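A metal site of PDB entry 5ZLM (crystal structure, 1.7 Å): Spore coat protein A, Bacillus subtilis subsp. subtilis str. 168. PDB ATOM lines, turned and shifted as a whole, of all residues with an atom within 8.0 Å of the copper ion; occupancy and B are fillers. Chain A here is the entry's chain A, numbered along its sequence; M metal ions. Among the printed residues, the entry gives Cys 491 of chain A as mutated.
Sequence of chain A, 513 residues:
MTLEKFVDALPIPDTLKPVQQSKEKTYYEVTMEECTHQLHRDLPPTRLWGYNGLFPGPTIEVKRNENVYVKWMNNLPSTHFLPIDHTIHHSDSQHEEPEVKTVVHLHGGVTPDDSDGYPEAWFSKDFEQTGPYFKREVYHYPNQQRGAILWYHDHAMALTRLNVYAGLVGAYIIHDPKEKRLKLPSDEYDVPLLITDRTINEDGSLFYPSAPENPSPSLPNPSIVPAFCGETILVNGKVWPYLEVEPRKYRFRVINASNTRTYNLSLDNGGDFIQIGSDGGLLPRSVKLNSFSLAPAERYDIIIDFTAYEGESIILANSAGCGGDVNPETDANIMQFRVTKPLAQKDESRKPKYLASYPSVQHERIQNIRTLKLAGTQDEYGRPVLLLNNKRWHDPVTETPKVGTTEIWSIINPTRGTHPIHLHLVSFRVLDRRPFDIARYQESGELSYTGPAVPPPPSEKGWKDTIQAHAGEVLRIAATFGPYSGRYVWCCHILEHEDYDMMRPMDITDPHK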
ATOM      1  N   PRO A 226      29.955   4.682  -1.386  1.00  0.00           N
ATOM      2  CA  PRO A 226      28.717   3.925  -1.649  1.00  0.00           C
ATOM      3  C   PRO A 226      28.921   2.526  -2.116  1.00  0.00           C
ATOM      4  O   PRO A 226      27.934   1.818  -2.270  1.00  0.00           O
ATOM      5  CB  PRO A 226      28.020   4.752  -2.759  1.00  0.00           C
ATOM      6  CG  PRO A 226      29.117   5.449  -3.423  1.00  0.00           C
ATOM      7  CD  PRO A 226      30.199   5.709  -2.410  1.00  0.00           C
ATOM      8  N   LEU A 374      13.029   0.932  -3.742  1.00  0.00           N
ATOM      9  CA  LEU A 374      14.452   1.186  -3.461  1.00  0.00           C
ATOM     10  C   LEU A 374      14.911   2.497  -4.094  1.00  0.00           C
ATOM     11  O   LEU A 374      14.852   2.651  -5.304  1.00  0.00           O
ATOM     12  CB  LEU A 374      15.273   0.027  -4.043  1.00  0.00           C
ATOM     13  CG  LEU A 374      14.812  -1.384  -3.670  1.00  0.00           C
ATOM     14  CD1 LEU A 374      15.762  -2.412  -4.260  1.00  0.00           C
ATOM     15  CD2 LEU A 374      14.682  -1.580  -2.183  1.00  0.00           C
ATOM     16  N   LEU A 386      21.056   5.944   0.578  1.00  0.00           N
ATOM     17  CA  LEU A 386      20.178   4.950  -0.034  1.00  0.00           C
ATOM     18  C   LEU A 386      19.111   4.520   0.972  1.00  0.00           C
ATOM     19  O   LEU A 386      19.448   4.249   2.122  1.00  0.00           O
ATOM     20  CB  LEU A 386      20.960   3.712  -0.493  1.00  0.00           C
ATOM     21  CG  LEU A 386      21.624   3.977  -1.829  1.00  0.00           C
ATOM     22  CD1 LEU A 386      22.840   3.124  -2.060  1.00  0.00           C
ATOM     23  CD2 LEU A 386      20.605   3.763  -2.957  1.00  0.00           C
ATOM     24  N   LEU A 387      17.840   4.493   0.551  1.00  0.00           N
ATOM     25  CA  LEU A 387      16.741   4.299   1.474  1.00  0.00           C
ATOM     26  C   LEU A 387      15.794   3.213   1.003  1.00  0.00           C
ATOM     27  O   LEU A 387      15.564   3.004  -0.220  1.00  0.00           O
ATOM     28  CB  LEU A 387      15.947   5.594   1.671  1.00  0.00           C
ATOM     29  CG  LEU A 387      16.669   6.861   2.057  1.00  0.00           C
ATOM     30  CD1 LEU A 387      15.686   8.032   2.125  1.00  0.00           C
ATOM     31  CD2 LEU A 387      17.345   6.712   3.391  1.00  0.00           C
ATOM     32  N   LEU A 388      15.229   2.519   1.996  1.00  0.00           N
ATOM     33  CA  LEU A 388      14.176   1.579   1.754  1.00  0.00           C
ATOM     34  C   LEU A 388      12.808   2.288   1.919  1.00  0.00           C
ATOM     35  O   LEU A 388      12.431   2.714   3.025  1.00  0.00           O
ATOM     36  CB  LEU A 388      14.248   0.424   2.749  1.00  0.00           C
ATOM     37  CG  LEU A 388      15.532  -0.432   2.645  1.00  0.00           C
ATOM     38  CD1 LEU A 388      15.589  -1.446   3.752  1.00  0.00           C
ATOM     39  CD2 LEU A 388      15.647  -1.105   1.283  1.00  0.00           C
ATOM     40  N   ASN A 413      12.685  -1.549  -7.985  1.00  0.00           N
ATOM     41  CA  ASN A 413      14.030  -1.011  -8.091  1.00  0.00           C
ATOM     42  C   ASN A 413      14.238  -0.141  -9.317  1.00  0.00           C
ATOM     43  O   ASN A 413      14.591  -0.647 -10.385  1.00  0.00           O
ATOM     44  CB  ASN A 413      15.084  -2.121  -8.115  1.00  0.00           C
ATOM     45  CG  ASN A 413      16.494  -1.577  -8.171  1.00  0.00           C
ATOM     46  OD1 ASN A 413      16.737  -0.363  -8.115  1.00  0.00           O
ATOM     47  ND2 ASN A 413      17.468  -2.472  -8.239  1.00  0.00           N
ATOM     48  N   THR A 415      16.640   2.099  -9.458  1.00  0.00           N
ATOM     49  CA  THR A 415      18.023   2.552  -9.443  1.00  0.00           C
ATOM     50  C   THR A 415      18.835   1.842 -10.548  1.00  0.00           C
ATOM     51  O   THR A 415      18.344   0.942 -11.227  1.00  0.00           O
ATOM     52  CB  THR A 415      18.683   2.334  -8.060  1.00  0.00           C
ATOM     53  OG1 THR A 415      19.049   0.948  -7.906  1.00  0.00           O
ATOM     54  CG2 THR A 415      17.737   2.753  -6.910  1.00  0.00           C
ATOM     55  N   GLY A 417      21.528  -0.135 -10.273  1.00  0.00           N
ATOM     56  CA  GLY A 417      22.187  -1.414  -9.981  1.00  0.00           C
ATOM     57  C   GLY A 417      21.341  -2.335  -9.146  1.00  0.00           C
ATOM     58  O   GLY A 417      20.260  -1.978  -8.715  1.00  0.00           O
ATOM     59  N   THR A 418      21.831  -3.559  -8.983  1.00  0.00           N
ATOM     60  CA  THR A 418      21.164  -4.571  -8.206  1.00  0.00           C
ATOM     61  C   THR A 418      21.385  -4.356  -6.708  1.00  0.00           C
ATOM     62  O   THR A 418      22.462  -3.950  -6.269  1.00  0.00           O
ATOM     63  CB  THR A 418      21.681  -5.976  -8.595  1.00  0.00           C
ATOM     64  OG1 THR A 418      21.442  -6.228  -9.985  1.00  0.00           O
ATOM     65  CG2 THR A 418      21.095  -7.084  -7.771  1.00  0.00           C
ATOM     66  N   HIS A 419      20.344  -4.611  -5.911  1.00  0.00           N
ATOM     67  CA  HIS A 419      20.450  -4.601  -4.429  1.00  0.00           C
ATOM     68  C   HIS A 419      20.084  -5.992  -3.956  1.00  0.00           C
ATOM     69  O   HIS A 419      19.044  -6.539  -4.304  1.00  0.00           O
ATOM     70  CB  HIS A 419      19.511  -3.572  -3.819  1.00  0.00           C
ATOM     71  CG  HIS A 419      19.785  -2.180  -4.257  1.00  0.00           C
ATOM     72  ND1 HIS A 419      20.721  -1.403  -3.638  1.00  0.00           N
ATOM     73  CD2 HIS A 419      19.284  -1.424  -5.277  1.00  0.00           C
ATOM     74  CE1 HIS A 419      20.773  -0.224  -4.206  1.00  0.00           C
ATOM     75  NE2 HIS A 419      19.928  -0.205  -5.219  1.00  0.00           N
ATOM     76  N   PRO A 420      20.956  -6.628  -3.122  1.00  0.00           N
ATOM     77  CA  PRO A 420      20.653  -7.892  -2.492  1.00  0.00           C
ATOM     78  C   PRO A 420      19.842  -7.682  -1.199  1.00  0.00           C
ATOM     79  O   PRO A 420      20.378  -7.328  -0.155  1.00  0.00           O
ATOM     80  CB  PRO A 420      22.069  -8.479  -2.234  1.00  0.00           C
ATOM     81  CG  PRO A 420      22.909  -7.267  -1.967  1.00  0.00           C
ATOM     82  CD  PRO A 420      22.324  -6.162  -2.787  1.00  0.00           C
ATOM     83  N   ILE A 421      18.535  -7.820  -1.311  1.00  0.00           N
ATOM     84  CA  ILE A 421      17.631  -7.540  -0.191  1.00  0.00           C
ATOM     85  C   ILE A 421      17.510  -8.741   0.755  1.00  0.00           C
ATOM     86  O   ILE A 421      17.259  -9.860   0.278  1.00  0.00           O
ATOM     87  CB  ILE A 421      16.243  -7.125  -0.736  1.00  0.00           C
ATOM     88  CG1 ILE A 421      16.388  -5.884  -1.600  1.00  0.00           C
ATOM     89  CG2 ILE A 421      15.286  -6.966   0.431  1.00  0.00           C
ATOM     90  CD1 ILE A 421      16.993  -4.665  -0.915  1.00  0.00           C
ATOM     91  N   ALA A 469      17.475  -7.965  -6.250  1.00  0.00           N
ATOM     92  CA  ALA A 469      16.484  -7.095  -6.893  1.00  0.00           C
ATOM     93  C   ALA A 469      17.205  -6.292  -7.918  1.00  0.00           C
ATOM     94  O   ALA A 469      17.868  -5.304  -7.611  1.00  0.00           O
ATOM     95  CB  ALA A 469      15.794  -6.212  -5.855  1.00  0.00           C
ATOM     96  N   CYS A 491      16.853  -5.308   5.052  1.00  0.00           N
ATOM     97  CA  CYS A 491      17.981  -4.462   4.659  1.00  0.00           C
ATOM     98  C   CYS A 491      18.518  -4.814   3.291  1.00  0.00           C
ATOM     99  O   CYS A 491      18.180  -5.883   2.727  1.00  0.00           O
ATOM    100  CB  CYS A 491      19.077  -4.577   5.702  1.00  0.00           C
ATOM    101  SG  CYS A 491      19.690  -6.269   5.957  1.00  0.00           S
ATOM    102  N   CYS A 492      19.291  -3.916   2.723  1.00  0.00           N
ATOM    103  CA  CYS A 492      20.141  -4.236   1.610  1.00  0.00           C
ATOM    104  C   CYS A 492      21.468  -4.704   2.181  1.00  0.00           C
ATOM    105  O   CYS A 492      22.019  -4.059   3.067  1.00  0.00           O
ATOM    106  CB  CYS A 492      20.362  -3.051   0.697  1.00  0.00           C
ATOM    107  SG  CYS A 492      21.591  -3.375  -0.571  1.00  0.00           S
ATOM    108  N   HIS A 493      21.967  -5.809   1.646  1.00  0.00           N
ATOM    109  CA  HIS A 493      23.209  -6.389   2.143  1.00  0.00           C
ATOM    110  C   HIS A 493      24.482  -5.938   1.441  1.00  0.00           C
ATOM    111  O   HIS A 493      25.578  -6.552   1.653  1.00  0.00           O
ATOM    112  CB  HIS A 493      23.113  -7.918   2.213  1.00  0.00           C
ATOM    113  CG  HIS A 493      23.688  -8.453   3.472  1.00  0.00           C
ATOM    114  ND1 HIS A 493      25.037  -8.602   3.638  1.00  0.00           N
ATOM    115  CD2 HIS A 493      23.117  -8.825   4.639  1.00  0.00           C
ATOM    116  CE1 HIS A 493      25.286  -9.057   4.843  1.00  0.00           C
ATOM    117  NE2 HIS A 493      24.144  -9.199   5.474  1.00  0.00           N
ATOM    118  N   ILE A 494      24.423  -4.886   0.645  1.00  0.00           N
ATOM    119  CA  ILE A 494      25.618  -4.154   0.262  1.00  0.00           C
ATOM    120  C   ILE A 494      25.910  -3.275   1.468  1.00  0.00           C
ATOM    121  O   ILE A 494      25.160  -2.349   1.789  1.00  0.00           O
ATOM    122  CB  ILE A 494      25.471  -3.324  -1.035  1.00  0.00           C
ATOM    123  CG1 ILE A 494      25.293  -4.248  -2.235  1.00  0.00           C
ATOM    124  CG2 ILE A 494      26.716  -2.410  -1.226  1.00  0.00           C
ATOM    125  CD1 ILE A 494      24.850  -3.533  -3.490  1.00  0.00           C
ATOM    126  N   LEU A 495      26.961  -3.602   2.205  1.00  0.00           N
ATOM    127  CA  LEU A 495      27.144  -3.010   3.507  1.00  0.00           C
ATOM    128  C   LEU A 495      27.321  -1.483   3.449  1.00  0.00           C
ATOM    129  O   LEU A 495      26.877  -0.788   4.346  1.00  0.00           O
ATOM    130  CB  LEU A 495      28.284  -3.706   4.263  1.00  0.00           C
ATOM    131  CG  LEU A 495      28.090  -5.229   4.376  1.00  0.00           C
ATOM    132  CD1 LEU A 495      29.225  -5.742   5.277  1.00  0.00           C
ATOM    133  CD2 LEU A 495      26.749  -5.598   5.008  1.00  0.00           C
ATOM    134  N   GLU A 496      27.978  -0.995   2.406  1.00  0.00           N
ATOM    135  CA  GLU A 496      28.134   0.438   2.180  1.00  0.00           C
ATOM    136  C   GLU A 496      26.762   1.142   2.019  1.00  0.00           C
ATOM    137  O   GLU A 496      26.648   2.351   2.345  1.00  0.00           O
ATOM    138  CB  GLU A 496      29.013   0.671   0.972  1.00  0.00           C
ATOM    139  CG  GLU A 496      30.507   0.448   1.211  1.00  0.00           C
ATOM    140  CD  GLU A 496      30.920  -1.004   1.451  1.00  0.00           C
ATOM    141  OE1 GLU A 496      30.228  -1.938   0.982  1.00  0.00           O
ATOM    142  OE2 GLU A 496      31.975  -1.195   2.141  1.00  0.00           O
ATOM    143  N   HIS A 497      25.767   0.401   1.518  1.00  0.00           N
ATOM    144  CA  HIS A 497      24.350   0.902   1.384  1.00  0.00           C
ATOM    145  C   HIS A 497      23.662   0.783   2.730  1.00  0.00           C
ATOM    146  O   HIS A 497      23.038   1.741   3.231  1.00  0.00           O
ATOM    147  CB  HIS A 497      23.535   0.131   0.350  1.00  0.00           C
ATOM    148  CG  HIS A 497      24.050   0.228  -1.047  1.00  0.00           C
ATOM    149  ND1 HIS A 497      23.431  -0.373  -2.113  1.00  0.00           N
ATOM    150  CD2 HIS A 497      25.122   0.877  -1.547  1.00  0.00           C
ATOM    151  CE1 HIS A 497      24.115  -0.100  -3.225  1.00  0.00           C
ATOM    152  NE2 HIS A 497      25.139   0.671  -2.901  1.00  0.00           N
ATOM    153  N   GLU A 498      23.745  -0.405   3.306  1.00  0.00           N
ATOM    154  CA  GLU A 498      23.145  -0.680   4.607  1.00  0.00           C
ATOM    155  C   GLU A 498      23.439   0.392   5.657  1.00  0.00           C
ATOM    156  O   GLU A 498      22.556   0.812   6.398  1.00  0.00           O
ATOM    157  CB  GLU A 498      23.639  -2.085   5.070  1.00  0.00           C
ATOM    158  CG  GLU A 498      22.870  -2.638   6.235  1.00  0.00           C
ATOM    159  CD  GLU A 498      23.386  -4.020   6.628  1.00  0.00           C
ATOM    160  OE1 GLU A 498      23.405  -4.939   5.806  1.00  0.00           O
ATOM    161  OE2 GLU A 498      23.753  -4.165   7.780  1.00  0.00           O
ATOM    162  N   MET A 502      20.287   2.072   4.143  1.00  0.00           N
ATOM    163  CA  MET A 502      19.370   1.168   3.460  1.00  0.00           C
ATOM    164  C   MET A 502      19.025  -0.072   4.332  1.00  0.00           C
ATOM    165  O   MET A 502      19.340  -1.210   4.004  1.00  0.00           O
ATOM    166  CB  MET A 502      19.942   0.803   2.109  1.00  0.00           C
ATOM    167  CG  MET A 502      18.942   0.341   1.077  1.00  0.00           C
ATOM    168  SD  MET A 502      19.703   0.204  -0.525  1.00  0.00           S
ATOM    169  CE  MET A 502      18.352  -0.338  -1.531  1.00  0.00           C
HETATM  170 CU    CU M   1      21.761  -1.638  -1.872  1.00  0.00          CU
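ND1 of His 419 lies close to SD of Met 502, 3.6 Å away. The side-chain hydroxyl (OG1) of Thr 415 lies within hydrogen-bond range of a ring nitrogen (NE2) of His 419 (3.1 Å). The backbone NH (N) of Ala 469 lies within hydrogen-bond range of the backbone carbonyl oxygen (O) of His 419 (2.9 Å). The backbone NH (N) of Met 502 lies within hydrogen-bond range of the backbone carbonyl oxygen (O) of His 497, 2.9 Å away. The backbone carbonyl oxygen (O) of Pro 226 lies close to a ring nitrogen (NE2) of His 497, 3.1 Å away. The backbone carbonyl oxygen (O) of Met 502 lies within hydrogen-bond range of the backbone NH (N) of Cys 492 (3.0 Å). The backbone NH (N) of Ile 494 lies close to the side-chain sulfur (SG) of Cys 492 (3.4 Å). The backbone NH (N) of Met 502 sits at hydrogen-bond distance from the backbone carbonyl oxygen (O) of Leu 386 (3.1 Å).
Residues that only touch the copper ion: Ile 494 (3.97 Å) and Met 502 (3.1 Å). Of the 22 residues printed, 5 come within 4 Å of the copper ion. Along chain A the residues within 4 Å of the copper ion span positions 419 to 502. The nearest printed residue that does not touch the copper ion is Pro 420 (4.6 Å).
The copper ion is bound by a ring nitrogen (ND1) of His 419 (2.1 Å), a ring nitrogen (ND1) of His 497 (2.1 Å) and the side-chain sulfur (SG) of Cys 492 (2.2 Å).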
